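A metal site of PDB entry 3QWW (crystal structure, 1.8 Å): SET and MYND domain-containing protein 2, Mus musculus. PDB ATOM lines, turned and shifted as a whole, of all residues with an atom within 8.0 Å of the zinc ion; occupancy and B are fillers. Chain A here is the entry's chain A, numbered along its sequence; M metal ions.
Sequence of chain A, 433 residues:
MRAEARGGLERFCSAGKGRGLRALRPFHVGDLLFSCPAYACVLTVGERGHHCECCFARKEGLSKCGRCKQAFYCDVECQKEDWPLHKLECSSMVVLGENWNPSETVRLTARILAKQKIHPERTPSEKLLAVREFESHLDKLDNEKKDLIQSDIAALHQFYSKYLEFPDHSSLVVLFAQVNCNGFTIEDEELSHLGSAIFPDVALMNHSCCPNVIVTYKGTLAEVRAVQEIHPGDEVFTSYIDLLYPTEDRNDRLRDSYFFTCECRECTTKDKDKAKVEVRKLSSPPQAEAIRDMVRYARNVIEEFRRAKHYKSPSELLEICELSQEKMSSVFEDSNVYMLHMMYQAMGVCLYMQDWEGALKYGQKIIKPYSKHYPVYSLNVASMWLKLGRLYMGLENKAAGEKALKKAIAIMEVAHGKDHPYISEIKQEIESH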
ATOM      1  N   HIS A  51     -26.560   6.038  12.977  1.00  0.00           N
ATOM      2  CA  HIS A  51     -25.708   5.116  13.732  1.00  0.00           C
ATOM      3  C   HIS A  51     -25.688   3.765  13.047  1.00  0.00           C
ATOM      4  O   HIS A  51     -26.697   3.387  12.451  1.00  0.00           O
ATOM      5  CB  HIS A  51     -26.264   4.912  15.164  1.00  0.00           C
ATOM      6  CG  HIS A  51     -26.092   6.088  16.067  1.00  0.00           C
ATOM      7  ND1 HIS A  51     -26.962   7.165  16.020  1.00  0.00           N
ATOM      8  CD2 HIS A  51     -25.156   6.326  16.996  1.00  0.00           C
ATOM      9  CE1 HIS A  51     -26.500   8.027  16.914  1.00  0.00           C
ATOM     10  NE2 HIS A  51     -25.421   7.551  17.528  1.00  0.00           N
ATOM     11  N   CYS A  52     -24.560   3.047  13.117  1.00  0.00           N
ATOM     12  CA  CYS A  52     -24.465   1.711  12.510  1.00  0.00           C
ATOM     13  C   CYS A  52     -25.466   0.766  13.194  1.00  0.00           C
ATOM     14  O   CYS A  52     -25.503   0.730  14.405  1.00  0.00           O
ATOM     15  CB  CYS A  52     -23.043   1.169  12.654  1.00  0.00           C
ATOM     16  SG  CYS A  52     -22.848  -0.573  12.187  1.00  0.00           S
ATOM     17  N   GLU A  53     -26.266   0.041  12.414  1.00  0.00           N
ATOM     18  CA  GLU A  53     -27.249  -0.917  12.907  1.00  0.00           C
ATOM     19  C   GLU A  53     -26.584  -2.020  13.766  1.00  0.00           C
ATOM     20  O   GLU A  53     -27.228  -2.574  14.647  1.00  0.00           O
ATOM     21  CB  GLU A  53     -27.995  -1.564  11.691  1.00  0.00           C
ATOM     22  CG  GLU A  53     -29.507  -1.574  11.779  1.00  0.00           C
ATOM     23  CD  GLU A  53     -30.231  -0.289  11.414  1.00  0.00           C
ATOM     24  OE1 GLU A  53     -29.745   0.476  10.545  1.00  0.00           O
ATOM     25  OE2 GLU A  53     -31.339  -0.086  11.962  1.00  0.00           O
ATOM     26  N   CYS A  54     -25.304  -2.349  13.518  1.00  0.00           N
ATOM     27  CA  CYS A  54     -24.622  -3.405  14.229  1.00  0.00           C
ATOM     28  C   CYS A  54     -23.953  -2.975  15.544  1.00  0.00           C
ATOM     29  O   CYS A  54     -24.235  -3.534  16.580  1.00  0.00           O
ATOM     30  CB  CYS A  54     -23.631  -4.106  13.313  1.00  0.00           C
ATOM     31  SG  CYS A  54     -22.710  -5.452  14.097  1.00  0.00           S
ATOM     32  N   CYS A  55     -23.033  -2.024  15.474  1.00  0.00           N
ATOM     33  CA  CYS A  55     -22.208  -1.629  16.605  1.00  0.00           C
ATOM     34  C   CYS A  55     -22.612  -0.305  17.253  1.00  0.00           C
ATOM     35  O   CYS A  55     -21.911   0.141  18.170  1.00  0.00           O
ATOM     36  CB  CYS A  55     -20.766  -1.581  16.134  1.00  0.00           C
ATOM     37  SG  CYS A  55     -20.404  -0.115  15.135  1.00  0.00           S
ATOM     38  N   PHE A  56     -23.611   0.406  16.695  1.00  0.00           N
ATOM     39  CA  PHE A  56     -24.133   1.692  17.159  1.00  0.00           C
ATOM     40  C   PHE A  56     -23.144   2.844  17.015  1.00  0.00           C
ATOM     41  O   PHE A  56     -23.383   3.895  17.600  1.00  0.00           O
ATOM     42  CB  PHE A  56     -24.695   1.616  18.611  1.00  0.00           C
ATOM     43  CG  PHE A  56     -25.937   0.759  18.877  1.00  0.00           C
ATOM     44  CD1 PHE A  56     -26.297  -0.270  18.009  1.00  0.00           C
ATOM     45  CD2 PHE A  56     -26.729   0.993  20.001  1.00  0.00           C
ATOM     46  CE1 PHE A  56     -27.414  -1.053  18.248  1.00  0.00           C
ATOM     47  CE2 PHE A  56     -27.863   0.212  20.241  1.00  0.00           C
ATOM     48  CZ  PHE A  56     -28.200  -0.813  19.374  1.00  0.00           C
ATOM     49  N   ALA A  57     -22.081   2.705  16.190  1.00  0.00           N
ATOM     50  CA  ALA A  57     -21.142   3.817  15.966  1.00  0.00           C
ATOM     51  C   ALA A  57     -21.849   4.981  15.269  1.00  0.00           C
ATOM     52  O   ALA A  57     -22.652   4.741  14.340  1.00  0.00           O
ATOM     53  CB  ALA A  57     -19.950   3.369  15.127  1.00  0.00           C
ATOM     54  N   ARG A  58     -21.601   6.221  15.753  1.00  0.00           N
ATOM     55  CA  ARG A  58     -22.143   7.454  15.177  1.00  0.00           C
ATOM     56  C   ARG A  58     -21.142   7.867  14.098  1.00  0.00           C
ATOM     57  O   ARG A  58     -20.023   8.286  14.424  1.00  0.00           O
ATOM     58  CB  ARG A  58     -22.271   8.550  16.255  1.00  0.00           C
ATOM     59  CG  ARG A  58     -22.974   9.813  15.763  1.00  0.00           C
ATOM     60  CD  ARG A  58     -23.234  10.829  16.866  1.00  0.00           C
ATOM     61  NE  ARG A  58     -22.002  11.437  17.367  1.00  0.00           N
ATOM     62  CZ  ARG A  58     -21.483  12.576  16.921  1.00  0.00           C
ATOM     63  NH1 ARG A  58     -22.070  13.243  15.930  1.00  0.00           N
ATOM     64  NH2 ARG A  58     -20.364  13.058  17.447  1.00  0.00           N
ATOM     65  N   LYS A  59     -21.496   7.642  12.837  1.00  0.00           N
ATOM     66  CA  LYS A  59     -20.622   7.951  11.708  1.00  0.00           C
ATOM     67  C   LYS A  59     -21.403   8.568  10.574  1.00  0.00           C
ATOM     68  O   LYS A  59     -22.570   8.234  10.352  1.00  0.00           O
ATOM     69  CB  LYS A  59     -19.919   6.677  11.197  1.00  0.00           C
ATOM     70  CG  LYS A  59     -18.734   6.225  12.027  1.00  0.00           C
ATOM     71  CD  LYS A  59     -18.114   4.960  11.474  1.00  0.00           C
ATOM     72  CE  LYS A  59     -17.023   4.432  12.376  1.00  0.00           C
ATOM     73  NZ  LYS A  59     -16.506   3.114  11.895  1.00  0.00           N
ATOM     74  N   LEU A  62     -22.347   6.183   6.282  1.00  0.00           N
ATOM     75  CA  LEU A  62     -22.539   4.750   6.554  1.00  0.00           C
ATOM     76  C   LEU A  62     -22.998   4.098   5.239  1.00  0.00           C
ATOM     77  O   LEU A  62     -23.788   4.690   4.506  1.00  0.00           O
ATOM     78  CB  LEU A  62     -23.644   4.534   7.610  1.00  0.00           C
ATOM     79  CG  LEU A  62     -23.339   4.986   9.030  1.00  0.00           C
ATOM     80  CD1 LEU A  62     -24.611   4.994   9.870  1.00  0.00           C
ATOM     81  CD2 LEU A  62     -22.295   4.095   9.690  1.00  0.00           C
ATOM     82  N   PHE A  72     -28.184   0.560   7.847  1.00  0.00           N
ATOM     83  CA  PHE A  72     -26.913   1.244   7.575  1.00  0.00           C
ATOM     84  C   PHE A  72     -25.789   0.707   8.452  1.00  0.00           C
ATOM     85  O   PHE A  72     -26.024   0.369   9.637  1.00  0.00           O
ATOM     86  CB  PHE A  72     -27.052   2.761   7.728  1.00  0.00           C
ATOM     87  CG  PHE A  72     -27.994   3.428   6.745  1.00  0.00           C
ATOM     88  CD1 PHE A  72     -29.378   3.319   6.882  1.00  0.00           C
ATOM     89  CD2 PHE A  72     -27.494   4.232   5.716  1.00  0.00           C
ATOM     90  CE1 PHE A  72     -30.236   3.973   5.992  1.00  0.00           C
ATOM     91  CE2 PHE A  72     -28.354   4.907   4.856  1.00  0.00           C
ATOM     92  CZ  PHE A  72     -29.718   4.765   4.989  1.00  0.00           C
ATOM     93  N   TYR A  73     -24.571   0.593   7.875  1.00  0.00           N
ATOM     94  CA  TYR A  73     -23.416  -0.025   8.515  1.00  0.00           C
ATOM     95  C   TYR A  73     -22.093   0.722   8.294  1.00  0.00           C
ATOM     96  O   TYR A  73     -21.933   1.409   7.279  1.00  0.00           O
ATOM     97  CB  TYR A  73     -23.260  -1.475   8.027  1.00  0.00           C
ATOM     98  CG  TYR A  73     -24.473  -2.364   8.260  1.00  0.00           C
ATOM     99  CD1 TYR A  73     -24.724  -2.935   9.501  1.00  0.00           C
ATOM    100  CD2 TYR A  73     -25.352  -2.662   7.214  1.00  0.00           C
ATOM    101  CE1 TYR A  73     -25.836  -3.755   9.704  1.00  0.00           C
ATOM    102  CE2 TYR A  73     -26.488  -3.443   7.416  1.00  0.00           C
ATOM    103  CZ  TYR A  73     -26.705  -4.019   8.655  1.00  0.00           C
ATOM    104  OH  TYR A  73     -27.782  -4.843   8.857  1.00  0.00           O
ATOM    105  N   CYS A  74     -21.154   0.572   9.250  1.00  0.00           N
ATOM    106  CA  CYS A  74     -19.780   1.096   9.244  1.00  0.00           C
ATOM    107  C   CYS A  74     -19.076   0.639   7.970  1.00  0.00           C
ATOM    108  O   CYS A  74     -18.433   1.440   7.261  1.00  0.00           O
ATOM    109  CB  CYS A  74     -19.025   0.564  10.459  1.00  0.00           C
ATOM    110  SG  CYS A  74     -19.524   1.331  12.016  1.00  0.00           S
ATOM    111  N   ASP A  75     -19.140  -0.662   7.727  1.00  0.00           N
ATOM    112  CA  ASP A  75     -18.463  -1.345   6.646  1.00  0.00           C
ATOM    113  C   ASP A  75     -19.099  -2.713   6.440  1.00  0.00           C
ATOM    114  O   ASP A  75     -20.053  -3.077   7.147  1.00  0.00           O
ATOM    115  CB  ASP A  75     -16.944  -1.482   6.977  1.00  0.00           C
ATOM    116  CG  ASP A  75     -16.587  -2.039   8.364  1.00  0.00           C
ATOM    117  OD1 ASP A  75     -17.481  -2.646   9.019  1.00  0.00           O
ATOM    118  OD2 ASP A  75     -15.428  -1.881   8.788  1.00  0.00           O
ATOM    119  N   GLU A  77     -17.895  -5.533   7.295  1.00  0.00           N
ATOM    120  CA  GLU A  77     -17.756  -6.362   8.500  1.00  0.00           C
ATOM    121  C   GLU A  77     -18.941  -6.223   9.467  1.00  0.00           C
ATOM    122  O   GLU A  77     -19.468  -7.239   9.909  1.00  0.00           O
ATOM    123  CB  GLU A  77     -16.411  -6.119   9.199  1.00  0.00           C
ATOM    124  CG  GLU A  77     -15.259  -6.591   8.330  1.00  0.00           C
ATOM    125  CD  GLU A  77     -14.638  -5.573   7.388  1.00  0.00           C
ATOM    126  OE1 GLU A  77     -15.289  -4.550   7.069  1.00  0.00           O
ATOM    127  OE2 GLU A  77     -13.489  -5.815   6.962  1.00  0.00           O
ATOM    128  N   CYS A  78     -19.392  -4.987   9.734  1.00  0.00           N
ATOM    129  CA  CYS A  78     -20.591  -4.773  10.562  1.00  0.00           C
ATOM    130  C   CYS A  78     -21.858  -5.348   9.848  1.00  0.00           C
ATOM    131  O   CYS A  78     -22.703  -5.971  10.490  1.00  0.00           O
ATOM    132  CB  CYS A  78     -20.762  -3.310  10.927  1.00  0.00           C
ATOM    133  SG  CYS A  78     -19.923  -2.823  12.477  1.00  0.00           S
ATOM    134  N   GLN A  79     -21.938  -5.189   8.529  1.00  0.00           N
ATOM    135  CA  GLN A  79     -23.074  -5.709   7.737  1.00  0.00           C
ATOM    136  C   GLN A  79     -23.180  -7.234   7.858  1.00  0.00           C
ATOM    137  O   GLN A  79     -24.282  -7.783   8.003  1.00  0.00           O
ATOM    138  CB  GLN A  79     -22.922  -5.281   6.269  1.00  0.00           C
ATOM    139  CG  GLN A  79     -23.987  -5.843   5.350  1.00  0.00           C
ATOM    140  CD  GLN A  79     -23.875  -5.262   3.972  1.00  0.00           C
ATOM    141  OE1 GLN A  79     -24.881  -5.049   3.284  1.00  0.00           O
ATOM    142  NE2 GLN A  79     -22.643  -4.931   3.581  1.00  0.00           N
ATOM    143  N   GLU A  81     -21.779  -9.151  10.314  1.00  0.00           N
ATOM    144  CA  GLU A  81     -22.103  -9.568  11.697  1.00  0.00           C
ATOM    145  C   GLU A  81     -23.616  -9.458  11.945  1.00  0.00           C
ATOM    146  O   GLU A  81     -24.211 -10.349  12.564  1.00  0.00           O
ATOM    147  CB  GLU A  81     -21.344  -8.709  12.716  1.00  0.00           C
ATOM    148  CG  GLU A  81     -21.422  -9.304  14.119  1.00  0.00           C
ATOM    149  CD  GLU A  81     -20.979  -8.399  15.244  1.00  0.00           C
ATOM    150  OE1 GLU A  81     -20.118  -7.525  15.014  1.00  0.00           O
ATOM    151  OE2 GLU A  81     -21.471  -8.598  16.386  1.00  0.00           O
HETATM  152 ZN    ZN M   1     -20.580  -0.758  12.867  1.00  0.00          ZN
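The side-chain sulfur (SG) of Cys 54 lies close to the backbone carbonyl oxygen (O) of Cys 78 (3.6 Å). The backbone NH (N) of Cys 78 lies within hydrogen-bond range of the side-chain carboxylate (OD1) of Asp 75 (3.1 Å). The backbone NH of Ala 57 sits close to the side-chain sulfur of Cys 55, 3.4 Å away. The side-chain sulfur (SG) of Cys 52 sits close to the backbone NH (N) of Cys 54, 3.3 Å away. N of Cys 52 lies within hydrogen-bond range of O of Ala 57 (2.8 Å). SG of Cys 74 lies close to NZ of Lys 59, 3.5 Å away.
Within 4 Å of the zinc ion: Cys 52, Cys 55, Cys 74 and Cys 78. The nearest printed residue that does not touch the zinc ion is Cys 54 (4.6 Å).
SG of Cys 78 binds the zinc ion. The zinc ion is bound by SG of Cys 55 (2.4 Å). The zinc ion is bound by SG of Cys 52, 2.4 Å away. The zinc ion is bound by SG of Cys 74, 2.5 Å away. The zinc ion has four donor atoms within binding distance.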
